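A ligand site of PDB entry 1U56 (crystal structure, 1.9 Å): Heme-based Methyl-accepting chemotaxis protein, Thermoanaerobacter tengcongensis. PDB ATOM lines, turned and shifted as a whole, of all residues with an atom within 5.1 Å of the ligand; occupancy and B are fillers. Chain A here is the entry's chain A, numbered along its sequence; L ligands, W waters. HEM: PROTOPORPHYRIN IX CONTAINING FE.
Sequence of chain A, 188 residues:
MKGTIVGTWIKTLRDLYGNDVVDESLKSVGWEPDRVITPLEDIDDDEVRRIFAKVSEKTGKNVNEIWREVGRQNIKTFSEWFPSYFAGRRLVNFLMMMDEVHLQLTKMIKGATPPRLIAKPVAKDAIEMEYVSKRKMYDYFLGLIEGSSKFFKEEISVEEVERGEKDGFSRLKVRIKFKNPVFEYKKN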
ATOM      1  N   MET A   1     -18.462  -5.824  18.192  1.00  0.00           N
ATOM      2  CA  MET A   1     -17.157  -5.338  17.625  1.00  0.00           C
ATOM      3  C   MET A   1     -17.398  -4.018  16.919  1.00  0.00           C
ATOM      4  O   MET A   1     -18.363  -3.885  16.159  1.00  0.00           O
ATOM      5  CB  MET A   1     -16.608  -6.357  16.631  1.00  0.00           C
ATOM      6  CG  MET A   1     -15.122  -6.234  16.370  1.00  0.00           C
ATOM      7  SD  MET A   1     -14.116  -6.752  17.801  1.00  0.00           S
ATOM      8  CE  MET A   1     -14.451  -8.496  17.882  1.00  0.00           C
ATOM      9  N   LYS A   2     -16.528  -3.025  17.152  1.00  0.00           N
ATOM     10  CA  LYS A   2     -16.684  -1.738  16.496  1.00  0.00           C
ATOM     11  C   LYS A   2     -16.868  -1.941  14.989  1.00  0.00           C
ATOM     12  O   LYS A   2     -16.029  -2.571  14.329  1.00  0.00           O
ATOM     13  CB  LYS A   2     -15.477  -0.839  16.777  1.00  0.00           C
ATOM     14  CG  LYS A   2     -15.568   0.514  16.101  1.00  0.00           C
ATOM     15  CD  LYS A   2     -14.468   1.452  16.543  1.00  0.00           C
ATOM     16  CE  LYS A   2     -14.409   2.684  15.649  1.00  0.00           C
ATOM     17  NZ  LYS A   2     -15.756   3.305  15.497  1.00  0.00           N
ATOM     18  N   ILE A   5     -14.127  -1.359  12.225  1.00  0.00           N
ATOM     19  CA  ILE A   5     -13.011  -2.308  12.266  1.00  0.00           C
ATOM     20  C   ILE A   5     -13.450  -3.572  11.533  1.00  0.00           C
ATOM     21  O   ILE A   5     -12.637  -4.211  10.857  1.00  0.00           O
ATOM     22  CB  ILE A   5     -12.605  -2.655  13.705  1.00  0.00           C
ATOM     23  CG1 ILE A   5     -12.310  -1.368  14.488  1.00  0.00           C
ATOM     24  CG2 ILE A   5     -11.385  -3.587  13.685  1.00  0.00           C
ATOM     25  CD1 ILE A   5     -11.175  -0.490  13.900  1.00  0.00           C
ATOM     26  N   TRP A   9     -11.828  -5.807   8.172  1.00  0.00           N
ATOM     27  CA  TRP A   9     -11.729  -7.256   8.036  1.00  0.00           C
ATOM     28  C   TRP A   9     -12.398  -7.718   6.735  1.00  0.00           C
ATOM     29  O   TRP A   9     -11.888  -8.593   6.048  1.00  0.00           O
ATOM     30  CB  TRP A   9     -12.399  -7.962   9.215  1.00  0.00           C
ATOM     31  CG  TRP A   9     -11.709  -7.683  10.513  1.00  0.00           C
ATOM     32  CD1 TRP A   9     -10.453  -7.166  10.683  1.00  0.00           C
ATOM     33  CD2 TRP A   9     -12.241  -7.894  11.828  1.00  0.00           C
ATOM     34  NE1 TRP A   9     -10.166  -7.045  12.034  1.00  0.00           N
ATOM     35  CE2 TRP A   9     -11.249  -7.481  12.753  1.00  0.00           C
ATOM     36  CE3 TRP A   9     -13.454  -8.391  12.315  1.00  0.00           C
ATOM     37  CZ2 TRP A   9     -11.443  -7.552  14.138  1.00  0.00           C
ATOM     38  CZ3 TRP A   9     -13.648  -8.461  13.700  1.00  0.00           C
ATOM     39  CH2 TRP A   9     -12.642  -8.039  14.597  1.00  0.00           C
ATOM     40  N   ILE A  75      -2.991  -5.070   8.874  1.00  0.00           N
ATOM     41  CA  ILE A  75      -2.187  -3.892   9.197  1.00  0.00           C
ATOM     42  C   ILE A  75      -2.142  -3.002   7.949  1.00  0.00           C
ATOM     43  O   ILE A  75      -2.291  -1.784   8.036  1.00  0.00           O
ATOM     44  CB  ILE A  75      -0.758  -4.292   9.626  1.00  0.00           C
ATOM     45  CG1 ILE A  75      -0.828  -5.039  10.961  1.00  0.00           C
ATOM     46  CG2 ILE A  75       0.135  -3.042   9.736  1.00  0.00           C
ATOM     47  CD1 ILE A  75      -1.392  -4.186  12.117  1.00  0.00           C
ATOM     48  N   PHE A  78      -5.393  -1.210   7.670  1.00  0.00           N
ATOM     49  CA  PHE A  78      -5.422  -0.130   8.659  1.00  0.00           C
ATOM     50  C   PHE A  78      -4.614   1.068   8.183  1.00  0.00           C
ATOM     51  O   PHE A  78      -5.025   2.213   8.367  1.00  0.00           O
ATOM     52  CB  PHE A  78      -4.827  -0.591   9.994  1.00  0.00           C
ATOM     53  CG  PHE A  78      -5.800  -1.328  10.880  1.00  0.00           C
ATOM     54  CD1 PHE A  78      -5.386  -2.470  11.572  1.00  0.00           C
ATOM     55  CD2 PHE A  78      -7.087  -0.858  11.063  1.00  0.00           C
ATOM     56  CE1 PHE A  78      -6.259  -3.133  12.432  1.00  0.00           C
ATOM     57  CE2 PHE A  78      -7.973  -1.503  11.927  1.00  0.00           C
ATOM     58  CZ  PHE A  78      -7.550  -2.643  12.613  1.00  0.00           C
ATOM     59  N   PHE A  82      -6.884   4.191   8.310  1.00  0.00           N
ATOM     60  CA  PHE A  82      -6.582   4.990   9.499  1.00  0.00           C
ATOM     61  C   PHE A  82      -5.117   5.396   9.416  1.00  0.00           C
ATOM     62  O   PHE A  82      -4.326   5.049  10.295  1.00  0.00           O
ATOM     63  CB  PHE A  82      -6.803   4.165  10.781  1.00  0.00           C
ATOM     64  CG  PHE A  82      -8.217   3.672  10.961  1.00  0.00           C
ATOM     65  CD1 PHE A  82      -8.741   2.667  10.149  1.00  0.00           C
ATOM     66  CD2 PHE A  82      -9.014   4.183  11.987  1.00  0.00           C
ATOM     67  CE1 PHE A  82     -10.028   2.188  10.344  1.00  0.00           C
ATOM     68  CE2 PHE A  82     -10.305   3.716  12.194  1.00  0.00           C
ATOM     69  CZ  PHE A  82     -10.805   2.706  11.379  1.00  0.00           C
ATOM     70  N   TYR A  85      -2.581   6.838  12.417  1.00  0.00           N
ATOM     71  CA  TYR A  85      -1.984   5.987  13.456  1.00  0.00           C
ATOM     72  C   TYR A  85      -0.624   5.458  13.051  1.00  0.00           C
ATOM     73  O   TYR A  85       0.065   4.842  13.843  1.00  0.00           O
ATOM     74  CB  TYR A  85      -2.899   4.801  13.787  1.00  0.00           C
ATOM     75  CG  TYR A  85      -4.210   5.201  14.422  1.00  0.00           C
ATOM     76  CD1 TYR A  85      -5.379   5.301  13.662  1.00  0.00           C
ATOM     77  CD2 TYR A  85      -4.270   5.544  15.765  1.00  0.00           C
ATOM     78  CE1 TYR A  85      -6.577   5.742  14.234  1.00  0.00           C
ATOM     79  CE2 TYR A  85      -5.459   6.000  16.352  1.00  0.00           C
ATOM     80  CZ  TYR A  85      -6.608   6.083  15.581  1.00  0.00           C
ATOM     81  OH  TYR A  85      -7.792   6.527  16.156  1.00  0.00           O
ATOM     82  N   PHE A  86      -0.240   5.703  11.799  1.00  0.00           N
ATOM     83  CA  PHE A  86       1.022   5.226  11.282  1.00  0.00           C
ATOM     84  C   PHE A  86       1.950   6.419  11.109  1.00  0.00           C
ATOM     85  O   PHE A  86       2.785   6.676  11.961  1.00  0.00           O
ATOM     86  CB  PHE A  86       0.771   4.473   9.971  1.00  0.00           C
ATOM     87  CG  PHE A  86      -0.043   3.215  10.145  1.00  0.00           C
ATOM     88  CD1 PHE A  86       0.574   1.986  10.357  1.00  0.00           C
ATOM     89  CD2 PHE A  86      -1.436   3.282  10.201  1.00  0.00           C
ATOM     90  CE1 PHE A  86      -0.182   0.838  10.604  1.00  0.00           C
ATOM     91  CE2 PHE A  86      -2.202   2.143  10.452  1.00  0.00           C
ATOM     92  CZ  PHE A  86      -1.580   0.925  10.656  1.00  0.00           C
ATOM     93  N   PHE A  94       4.468   2.449  17.889  1.00  0.00           N
ATOM     94  CA  PHE A  94       3.184   1.957  17.403  1.00  0.00           C
ATOM     95  C   PHE A  94       2.585   0.969  18.404  1.00  0.00           C
ATOM     96  O   PHE A  94       1.471   1.157  18.897  1.00  0.00           O
ATOM     97  CB  PHE A  94       3.371   1.258  16.049  1.00  0.00           C
ATOM     98  CG  PHE A  94       2.090   0.777  15.426  1.00  0.00           C
ATOM     99  CD1 PHE A  94       1.154   1.688  14.917  1.00  0.00           C
ATOM    100  CD2 PHE A  94       1.831  -0.582  15.311  1.00  0.00           C
ATOM    101  CE1 PHE A  94      -0.032   1.225  14.318  1.00  0.00           C
ATOM    102  CE2 PHE A  94       0.644  -1.044  14.726  1.00  0.00           C
ATOM    103  CZ  PHE A  94      -0.276  -0.138  14.220  1.00  0.00           C
ATOM    104  N   LEU A  95       3.333  -0.074  18.711  1.00  0.00           N
ATOM    105  CA  LEU A  95       2.878  -1.102  19.628  1.00  0.00           C
ATOM    106  C   LEU A  95       2.480  -0.587  21.014  1.00  0.00           C
ATOM    107  O   LEU A  95       1.433  -0.952  21.535  1.00  0.00           O
ATOM    108  CB  LEU A  95       3.938  -2.198  19.752  1.00  0.00           C
ATOM    109  CG  LEU A  95       4.231  -2.977  18.450  1.00  0.00           C
ATOM    110  CD1 LEU A  95       5.319  -4.005  18.698  1.00  0.00           C
ATOM    111  CD2 LEU A  95       2.955  -3.663  17.975  1.00  0.00           C
ATOM    112  N   MET A  98      -1.004   1.128  21.152  1.00  0.00           N
ATOM    113  CA  MET A  98      -2.233   0.368  20.930  1.00  0.00           C
ATOM    114  C   MET A  98      -3.239   0.281  22.082  1.00  0.00           C
ATOM    115  O   MET A  98      -4.432   0.418  21.853  1.00  0.00           O
ATOM    116  CB  MET A  98      -1.890  -1.041  20.446  1.00  0.00           C
ATOM    117  CG  MET A  98      -1.254  -1.054  19.065  1.00  0.00           C
ATOM    118  SD  MET A  98      -2.384  -0.385  17.807  1.00  0.00           S
ATOM    119  CE  MET A  98      -2.060   1.378  17.859  1.00  0.00           C
ATOM    120  N   VAL A 101      -5.196   3.375  22.174  1.00  0.00           N
ATOM    121  CA  VAL A 101      -6.001   3.487  20.957  1.00  0.00           C
ATOM    122  C   VAL A 101      -7.289   2.676  21.035  1.00  0.00           C
ATOM    123  O   VAL A 101      -8.352   3.154  20.636  1.00  0.00           O
ATOM    124  CB  VAL A 101      -5.183   3.030  19.712  1.00  0.00           C
ATOM    125  CG1 VAL A 101      -6.107   2.812  18.520  1.00  0.00           C
ATOM    126  CG2 VAL A 101      -4.146   4.099  19.367  1.00  0.00           C
ATOM    127  N   HIS A 102      -7.206   1.441  21.545  1.00  0.00           N
ATOM    128  CA  HIS A 102      -8.393   0.606  21.632  1.00  0.00           C
ATOM    129  C   HIS A 102      -9.407   1.133  22.649  1.00  0.00           C
ATOM    130  O   HIS A 102     -10.620   0.978  22.461  1.00  0.00           O
ATOM    131  CB  HIS A 102      -7.999  -0.841  21.950  1.00  0.00           C
ATOM    132  CG  HIS A 102      -7.350  -1.554  20.809  1.00  0.00           C
ATOM    133  ND1 HIS A 102      -6.086  -1.227  20.357  1.00  0.00           N
ATOM    134  CD2 HIS A 102      -7.813  -2.498  19.954  1.00  0.00           C
ATOM    135  CE1 HIS A 102      -5.810  -1.943  19.282  1.00  0.00           C
ATOM    136  NE2 HIS A 102      -6.838  -2.720  19.016  1.00  0.00           N
ATOM    137  N   LEU A 105     -11.164   4.253  20.738  1.00  0.00           N
ATOM    138  CA  LEU A 105     -12.115   3.925  19.685  1.00  0.00           C
ATOM    139  C   LEU A 105     -13.346   3.171  20.159  1.00  0.00           C
ATOM    140  O   LEU A 105     -14.282   2.963  19.381  1.00  0.00           O
ATOM    141  CB  LEU A 105     -11.410   3.135  18.568  1.00  0.00           C
ATOM    142  CG  LEU A 105     -10.259   3.877  17.884  1.00  0.00           C
ATOM    143  CD1 LEU A 105      -9.642   3.025  16.778  1.00  0.00           C
ATOM    144  CD2 LEU A 105     -10.771   5.192  17.323  1.00  0.00           C
ATOM    145  N   THR A 106     -13.382   2.755  21.413  1.00  0.00           N
ATOM    146  CA  THR A 106     -14.548   2.023  21.921  1.00  0.00           C
ATOM    147  C   THR A 106     -15.196   2.810  23.061  1.00  0.00           C
ATOM    148  O   THR A 106     -16.157   2.337  23.685  1.00  0.00           O
ATOM    149  CB  THR A 106     -14.165   0.618  22.456  1.00  0.00           C
ATOM    150  OG1 THR A 106     -13.225   0.737  23.525  1.00  0.00           O
ATOM    151  CG2 THR A 106     -13.547  -0.226  21.334  1.00  0.00           C
ATOM    152  N   THR A 113     -16.172  -3.460  25.299  1.00  0.00           N
ATOM    153  CA  THR A 113     -15.277  -4.426  25.924  1.00  0.00           C
ATOM    154  C   THR A 113     -14.067  -4.626  25.007  1.00  0.00           C
ATOM    155  O   THR A 113     -13.880  -5.703  24.433  1.00  0.00           O
ATOM    156  CB  THR A 113     -15.972  -5.790  26.163  1.00  0.00           C
ATOM    157  OG1 THR A 113     -16.359  -6.361  24.905  1.00  0.00           O
ATOM    158  CG2 THR A 113     -17.206  -5.623  27.045  1.00  0.00           C
ATOM    159  N   PRO A 114     -13.240  -3.581  24.847  1.00  0.00           N
ATOM    160  CA  PRO A 114     -12.062  -3.686  23.985  1.00  0.00           C
ATOM    161  C   PRO A 114     -10.970  -4.537  24.614  1.00  0.00           C
ATOM    162  O   PRO A 114     -10.890  -4.666  25.847  1.00  0.00           O
ATOM    163  CB  PRO A 114     -11.622  -2.234  23.861  1.00  0.00           C
ATOM    164  CG  PRO A 114     -11.880  -1.724  25.258  1.00  0.00           C
ATOM    165  CD  PRO A 114     -13.280  -2.264  25.510  1.00  0.00           C
ATOM    166  N   PRO A 115     -10.111  -5.128  23.779  1.00  0.00           N
ATOM    167  CA  PRO A 115      -9.035  -5.944  24.329  1.00  0.00           C
ATOM    168  C   PRO A 115      -8.038  -4.999  24.980  1.00  0.00           C
ATOM    169  O   PRO A 115      -7.874  -3.855  24.549  1.00  0.00           O
ATOM    170  CB  PRO A 115      -8.438  -6.593  23.087  1.00  0.00           C
ATOM    171  CG  PRO A 115      -8.612  -5.507  22.045  1.00  0.00           C
ATOM    172  CD  PRO A 115     -10.029  -5.047  22.307  1.00  0.00           C
ATOM    173  N   LEU A 117      -4.161  -4.227  25.724  1.00  0.00           N
ATOM    174  CA  LEU A 117      -2.908  -4.601  25.085  1.00  0.00           C
ATOM    175  C   LEU A 117      -1.698  -3.917  25.717  1.00  0.00           C
ATOM    176  O   LEU A 117      -0.810  -3.422  25.023  1.00  0.00           O
ATOM    177  CB  LEU A 117      -2.979  -4.227  23.599  1.00  0.00           C
ATOM    178  CG  LEU A 117      -4.217  -4.776  22.875  1.00  0.00           C
ATOM    179  CD1 LEU A 117      -4.395  -4.084  21.530  1.00  0.00           C
ATOM    180  CD2 LEU A 117      -4.058  -6.268  22.694  1.00  0.00           C
ATOM    181  N   MET A 129       4.229  -7.682  25.814  1.00  0.00           N
ATOM    182  CA  MET A 129       2.892  -7.229  25.505  1.00  0.00           C
ATOM    183  C   MET A 129       1.886  -8.285  25.952  1.00  0.00           C
ATOM    184  O   MET A 129       2.012  -9.459  25.590  1.00  0.00           O
ATOM    185  CB  MET A 129       2.734  -6.964  24.007  1.00  0.00           C
ATOM    186  CG  MET A 129       1.390  -6.380  23.616  1.00  0.00           C
ATOM    187  SD  MET A 129       1.378  -5.841  21.894  1.00  0.00           S
ATOM    188  CE  MET A 129       2.078  -4.225  22.049  1.00  0.00           C
ATOM    189  N   TYR A 131      -2.029  -9.517  25.993  1.00  0.00           N
ATOM    190  CA  TYR A 131      -3.360  -9.429  25.415  1.00  0.00           C
ATOM    191  C   TYR A 131      -4.315  -9.944  26.483  1.00  0.00           C
ATOM    192  O   TYR A 131      -4.102 -11.025  27.034  1.00  0.00           O
ATOM    193  CB  TYR A 131      -3.453 -10.328  24.179  1.00  0.00           C
ATOM    194  CG  TYR A 131      -4.866 -10.628  23.724  1.00  0.00           C
ATOM    195  CD1 TYR A 131      -5.619  -9.678  23.033  1.00  0.00           C
ATOM    196  CD2 TYR A 131      -5.446 -11.878  23.963  1.00  0.00           C
ATOM    197  CE1 TYR A 131      -6.904  -9.964  22.594  1.00  0.00           C
ATOM    198  CE2 TYR A 131      -6.739 -12.165  23.530  1.00  0.00           C
ATOM    199  CZ  TYR A 131      -7.467 -11.198  22.840  1.00  0.00           C
ATOM    200  OH  TYR A 131      -8.754 -11.460  22.419  1.00  0.00           O
ATOM    201  N   SER A 133      -8.570 -10.273  27.043  1.00  0.00           N
ATOM    202  CA  SER A 133      -9.904 -10.098  26.489  1.00  0.00           C
ATOM    203  C   SER A 133     -10.811 -11.309  26.652  1.00  0.00           C
ATOM    204  O   SER A 133     -10.347 -12.442  26.725  1.00  0.00           O
ATOM    205  CB  SER A 133      -9.812  -9.801  24.984  1.00  0.00           C
ATOM    206  OG  SER A 133     -11.108  -9.810  24.400  1.00  0.00           O
ATOM    207  N   ARG A 135     -12.696 -12.329  24.402  1.00  0.00           N
ATOM    208  CA  ARG A 135     -12.804 -12.953  23.079  1.00  0.00           C
ATOM    209  C   ARG A 135     -11.772 -13.998  22.654  1.00  0.00           C
ATOM    210  O   ARG A 135     -11.998 -14.720  21.695  1.00  0.00           O
ATOM    211  CB  ARG A 135     -12.848 -11.849  22.008  1.00  0.00           C
ATOM    212  CG  ARG A 135     -13.998 -10.853  22.187  1.00  0.00           C
ATOM    213  CD  ARG A 135     -14.202 -10.040  20.924  1.00  0.00           C
ATOM    214  NE  ARG A 135     -15.214  -8.995  21.057  1.00  0.00           N
ATOM    215  CZ  ARG A 135     -14.950  -7.720  21.356  1.00  0.00           C
ATOM    216  NH1 ARG A 135     -13.700  -7.325  21.548  1.00  0.00           N
ATOM    217  NH2 ARG A 135     -15.933  -6.842  21.435  1.00  0.00           N
ATOM    218  N   MET A 137      -8.964 -13.960  20.965  1.00  0.00           N
ATOM    219  CA  MET A 137      -8.575 -13.894  19.563  1.00  0.00           C
ATOM    220  C   MET A 137      -7.046 -13.897  19.432  1.00  0.00           C
ATOM    221  O   MET A 137      -6.441 -12.981  18.885  1.00  0.00           O
ATOM    222  CB  MET A 137      -9.200 -12.650  18.932  1.00  0.00           C
ATOM    223  CG  MET A 137     -10.732 -12.816  18.797  1.00  0.00           C
ATOM    224  SD  MET A 137     -11.654 -11.414  18.129  1.00  0.00           S
ATOM    225  CE  MET A 137     -10.947 -11.349  16.401  1.00  0.00           C
ATOM    226  N   TYR A 140      -5.532 -13.681  15.764  1.00  0.00           N
ATOM    227  CA  TYR A 140      -5.642 -12.364  15.154  1.00  0.00           C
ATOM    228  C   TYR A 140      -4.552 -11.504  15.777  1.00  0.00           C
ATOM    229  O   TYR A 140      -3.809 -10.827  15.077  1.00  0.00           O
ATOM    230  CB  TYR A 140      -7.021 -11.747  15.423  1.00  0.00           C
ATOM    231  CG  TYR A 140      -7.231 -10.367  14.842  1.00  0.00           C
ATOM    232  CD1 TYR A 140      -6.998 -10.096  13.473  1.00  0.00           C
ATOM    233  CD2 TYR A 140      -7.666  -9.328  15.647  1.00  0.00           C
ATOM    234  CE1 TYR A 140      -7.210  -8.812  12.955  1.00  0.00           C
ATOM    235  CE2 TYR A 140      -7.883  -8.054  15.136  1.00  0.00           C
ATOM    236  CZ  TYR A 140      -7.648  -7.799  13.798  1.00  0.00           C
ATOM    237  OH  TYR A 140      -7.791  -6.520  13.333  1.00  0.00           O
ATOM    238  N   PHE A 141      -4.470 -11.543  17.107  1.00  0.00           N
ATOM    239  CA  PHE A 141      -3.451 -10.795  17.864  1.00  0.00           C
ATOM    240  C   PHE A 141      -2.032 -11.043  17.354  1.00  0.00           C
ATOM    241  O   PHE A 141      -1.289 -10.096  17.044  1.00  0.00           O
ATOM    242  CB  PHE A 141      -3.540 -11.201  19.341  1.00  0.00           C
ATOM    243  CG  PHE A 141      -2.450 -10.615  20.206  1.00  0.00           C
ATOM    244  CD1 PHE A 141      -2.430  -9.257  20.506  1.00  0.00           C
ATOM    245  CD2 PHE A 141      -1.459 -11.436  20.732  1.00  0.00           C
ATOM    246  CE1 PHE A 141      -1.430  -8.732  21.332  1.00  0.00           C
ATOM    247  CE2 PHE A 141      -0.457 -10.922  21.559  1.00  0.00           C
ATOM    248  CZ  PHE A 141      -0.450  -9.567  21.857  1.00  0.00           C
ATOM    249  N   LEU A 144      -1.475  -9.739  13.735  1.00  0.00           N
ATOM    250  CA  LEU A 144      -1.317  -8.291  13.646  1.00  0.00           C
ATOM    251  C   LEU A 144       0.122  -7.901  14.036  1.00  0.00           C
ATOM    252  O   LEU A 144       0.707  -6.984  13.465  1.00  0.00           O
ATOM    253  CB  LEU A 144      -2.325  -7.590  14.570  1.00  0.00           C
ATOM    254  CG  LEU A 144      -3.792  -7.634  14.105  1.00  0.00           C
ATOM    255  CD1 LEU A 144      -4.703  -7.349  15.274  1.00  0.00           C
ATOM    256  CD2 LEU A 144      -4.007  -6.621  13.002  1.00  0.00           C
ATOM    257  N   ILE A 145       0.695  -8.613  15.004  1.00  0.00           N
ATOM    258  CA  ILE A 145       2.058  -8.301  15.414  1.00  0.00           C
ATOM    259  C   ILE A 145       3.017  -8.641  14.281  1.00  0.00           C
ATOM    260  O   ILE A 145       3.906  -7.848  13.952  1.00  0.00           O
ATOM    261  CB  ILE A 145       2.431  -9.067  16.701  1.00  0.00           C
ATOM    262  CG1 ILE A 145       1.595  -8.543  17.870  1.00  0.00           C
ATOM    263  CG2 ILE A 145       3.923  -8.873  17.014  1.00  0.00           C
ATOM    264  CD1 ILE A 145       1.743  -9.324  19.166  1.00  0.00           C
ATOM    265  N   SER A 148       2.646  -6.131  11.605  1.00  0.00           N
ATOM    266  CA  SER A 148       3.195  -4.851  11.998  1.00  0.00           C
ATOM    267  C   SER A 148       4.690  -4.859  11.697  1.00  0.00           C
ATOM    268  O   SER A 148       5.224  -3.867  11.218  1.00  0.00           O
ATOM    269  CB  SER A 148       2.959  -4.592  13.494  1.00  0.00           C
ATOM    270  OG  SER A 148       1.586  -4.371  13.755  1.00  0.00           O
HETATM  271  CHA HEM L   1      -9.898  -5.277  17.740  1.00  0.00           C
HETATM  272  CHB HEM L   1      -8.632  -0.762  16.484  1.00  0.00           C
HETATM  273  CHC HEM L   1      -4.147  -2.399  15.740  1.00  0.00           C
HETATM  274  CHD HEM L   1      -5.231  -6.220  18.577  1.00  0.00           C
HETATM  275  C1A HEM L   1      -9.939  -3.891  17.525  1.00  0.00           C
HETATM  276  C2A HEM L   1     -11.098  -3.044  17.765  1.00  0.00           C
HETATM  277  C3A HEM L   1     -10.665  -1.769  17.525  1.00  0.00           C
HETATM  278  C4A HEM L   1      -9.342  -1.838  17.051  1.00  0.00           C
HETATM  279  CMA HEM L   1     -11.420  -0.469  17.789  1.00  0.00           C
HETATM  280  CAA HEM L   1     -12.513  -3.472  18.159  1.00  0.00           C
HETATM  281  CBA HEM L   1     -12.610  -3.599  19.686  1.00  0.00           C
HETATM  282  CGA HEM L   1     -14.037  -3.751  20.188  1.00  0.00           C
HETATM  283  O1A HEM L   1     -14.211  -4.120  21.375  1.00  0.00           O
HETATM  284  O2A HEM L   1     -14.993  -3.483  19.413  1.00  0.00           O
HETATM  285  C1B HEM L   1      -7.342  -0.887  15.977  1.00  0.00           C
HETATM  286  C2B HEM L   1      -6.648   0.108  15.188  1.00  0.00           C
HETATM  287  C3B HEM L   1      -5.422  -0.396  14.893  1.00  0.00           C
HETATM  288  C4B HEM L   1      -5.347  -1.668  15.579  1.00  0.00           C
HETATM  289  CMB HEM L   1      -7.231   1.424  14.682  1.00  0.00           C
HETATM  290  CAB HEM L   1      -4.388   0.080  14.041  1.00  0.00           C
HETATM  291  CBB HEM L   1      -4.106   1.464  13.681  1.00  0.00           C
HETATM  292  C1C HEM L   1      -4.014  -3.498  16.635  1.00  0.00           C
HETATM  293  C2C HEM L   1      -2.751  -4.120  16.984  1.00  0.00           C
HETATM  294  C3C HEM L   1      -3.036  -5.163  17.853  1.00  0.00           C
HETATM  295  C4C HEM L   1      -4.507  -5.202  17.955  1.00  0.00           C
HETATM  296  CMC HEM L   1      -1.414  -3.797  16.319  1.00  0.00           C
HETATM  297  CAC HEM L   1      -2.197  -6.089  18.495  1.00  0.00           C
HETATM  298  CBC HEM L   1      -0.745  -5.961  18.652  1.00  0.00           C
HETATM  299  C1D HEM L   1      -6.617  -6.357  18.451  1.00  0.00           C
HETATM  300  C2D HEM L   1      -7.357  -7.531  18.839  1.00  0.00           C
HETATM  301  C3D HEM L   1      -8.673  -7.306  18.569  1.00  0.00           C
HETATM  302  C4D HEM L   1      -8.740  -5.963  18.062  1.00  0.00           C
HETATM  303  CMD HEM L   1      -6.745  -8.833  19.319  1.00  0.00           C
HETATM  304  CAD HEM L   1      -9.807  -8.338  18.515  1.00  0.00           C
HETATM  305  CBD HEM L   1     -10.901  -8.217  19.608  1.00  0.00           C
HETATM  306  CGD HEM L   1     -10.515  -8.881  20.927  1.00  0.00           C
HETATM  307  O1D HEM L   1      -9.558  -9.674  20.956  1.00  0.00           O
HETATM  308  O2D HEM L   1     -11.189  -8.631  21.951  1.00  0.00           O
HETATM  309  NA  HEM L   1      -8.862  -3.135  17.117  1.00  0.00           N
HETATM  310  NB  HEM L   1      -6.551  -2.014  16.149  1.00  0.00           N
HETATM  311  NC  HEM L   1      -5.080  -4.146  17.246  1.00  0.00           N
HETATM  312  ND  HEM L   1      -7.459  -5.388  17.955  1.00  0.00           N
HETATM  313 FE   HEM L   1      -6.987  -3.689  17.099  1.00  0.00          FE
HETATM  314  O   HOH W   1     -13.110  -8.143  24.723  1.00  0.00           O
HETATM  315  O   HOH W   2     -17.341  -3.925  20.837  1.00  0.00           O
HETATM  316  O   HOH W   3     -15.969  -3.174  22.818  1.00  0.00           O
HETATM  317  O   HOH W   4      -7.206  -4.613  15.247  1.00  0.00           O
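FE of the ligand is bound by NE2 of His 102, at 2.2 Å. The side-chain hydroxyl (OH) of Tyr 131 lies within hydrogen-bond range of an oxygen (O1D) of the ligand, at 2.4 Å. OG of Ser 133 is in hydrogen-bond range of O2D of the ligand (2.7 Å). An oxygen (O2A) of the ligand sits at hydrogen-bond distance from the backbone NH (N) of Lys 2 (2.8 Å). NH1 of Arg 135 is in salt-bridge range of O2D of the ligand, at 2.9 Å.
Water W3 bridges O1A of the ligand (2.5 Å) and N of Thr 113 (2.5 Å). Water W2 lies within hydrogen-bond range of an oxygen (O2A) of the ligand, the guanidinium group (NH2) of Arg 135 and the backbone NH (N) of Met 1. Water W1 lies within hydrogen-bond range of O of Thr 113 (2.6 Å), OG of Ser 133 (2.6 Å), NH1 of Arg 135 (3.3 Å) and O2D of the ligand (3.4 Å).
The backbone carbonyl oxygen (O) of Met 98 sits at hydrogen-bond distance from a ring nitrogen (ND1) of His 102, 2.8 Å away. The backbone carbonyl oxygen of His 102 sits at hydrogen-bond distance from the side-chain hydroxyl of Thr 106. OG of Ser 133 lies close to OH of Tyr 131, 3.5 Å away. The side-chain hydroxyl (OH) of Tyr 131 lies within hydrogen-bond range of the backbone NH (N) of Met 137. The side-chain hydroxyl (OG) of Ser 133 is in hydrogen-bond range of the backbone NH (N) of Arg 135. The backbone carbonyl oxygen (O) of Thr 113 lies within hydrogen-bond range of the guanidinium group (NH1) of Arg 135 (3.3 Å). The backbone carbonyl oxygen (O) of Leu 144 sits at hydrogen-bond distance from the side-chain hydroxyl (OG) of Ser 148, at 2.8 Å. The indole nitrogen (NE1) of Trp 9 sits at hydrogen-bond distance from the side-chain hydroxyl (OH) of Tyr 140 (2.8 Å).
O2A of the ligand sits close to SD of Met 1, at 3.7 Å. O of Thr 113 sits close to O1A of the ligand, at 3.5 Å. CG1 of Ile 5 touches C3A of the ligand, at 3.5 Å. CE1 of Phe 78 touches C4B of the ligand, at 3.6 Å. Tyr 85 touches the ligand (CB to CBB, 3.6 Å). Phe 86 touches the ligand (CE2 to CBB, 3.8 Å). CE2 of Phe 94 touches CMC of the ligand, 3.8 Å away. Met 98 touches the ligand. Leu 105 touches the ligand. CG2 of Thr 106 touches CGA of the ligand, at 3.7 Å. Pro 114 touches the ligand. CB of Pro 115 touches O2D of the ligand (3.6 Å). Leu 117 touches the ligand. Met 129 touches the ligand. Met 137 touches the ligand (SD to CBD, 3.6 Å). CE2 of Tyr 140 touches C3D of the ligand (3.6 Å). CD1 of Phe 141 touches CAC of the ligand, at 3.8 Å. Leu 144 touches the ligand (CD1 to C4C, 3.4 Å). Ile 145 touches the ligand. Ser 148 touches the ligand.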
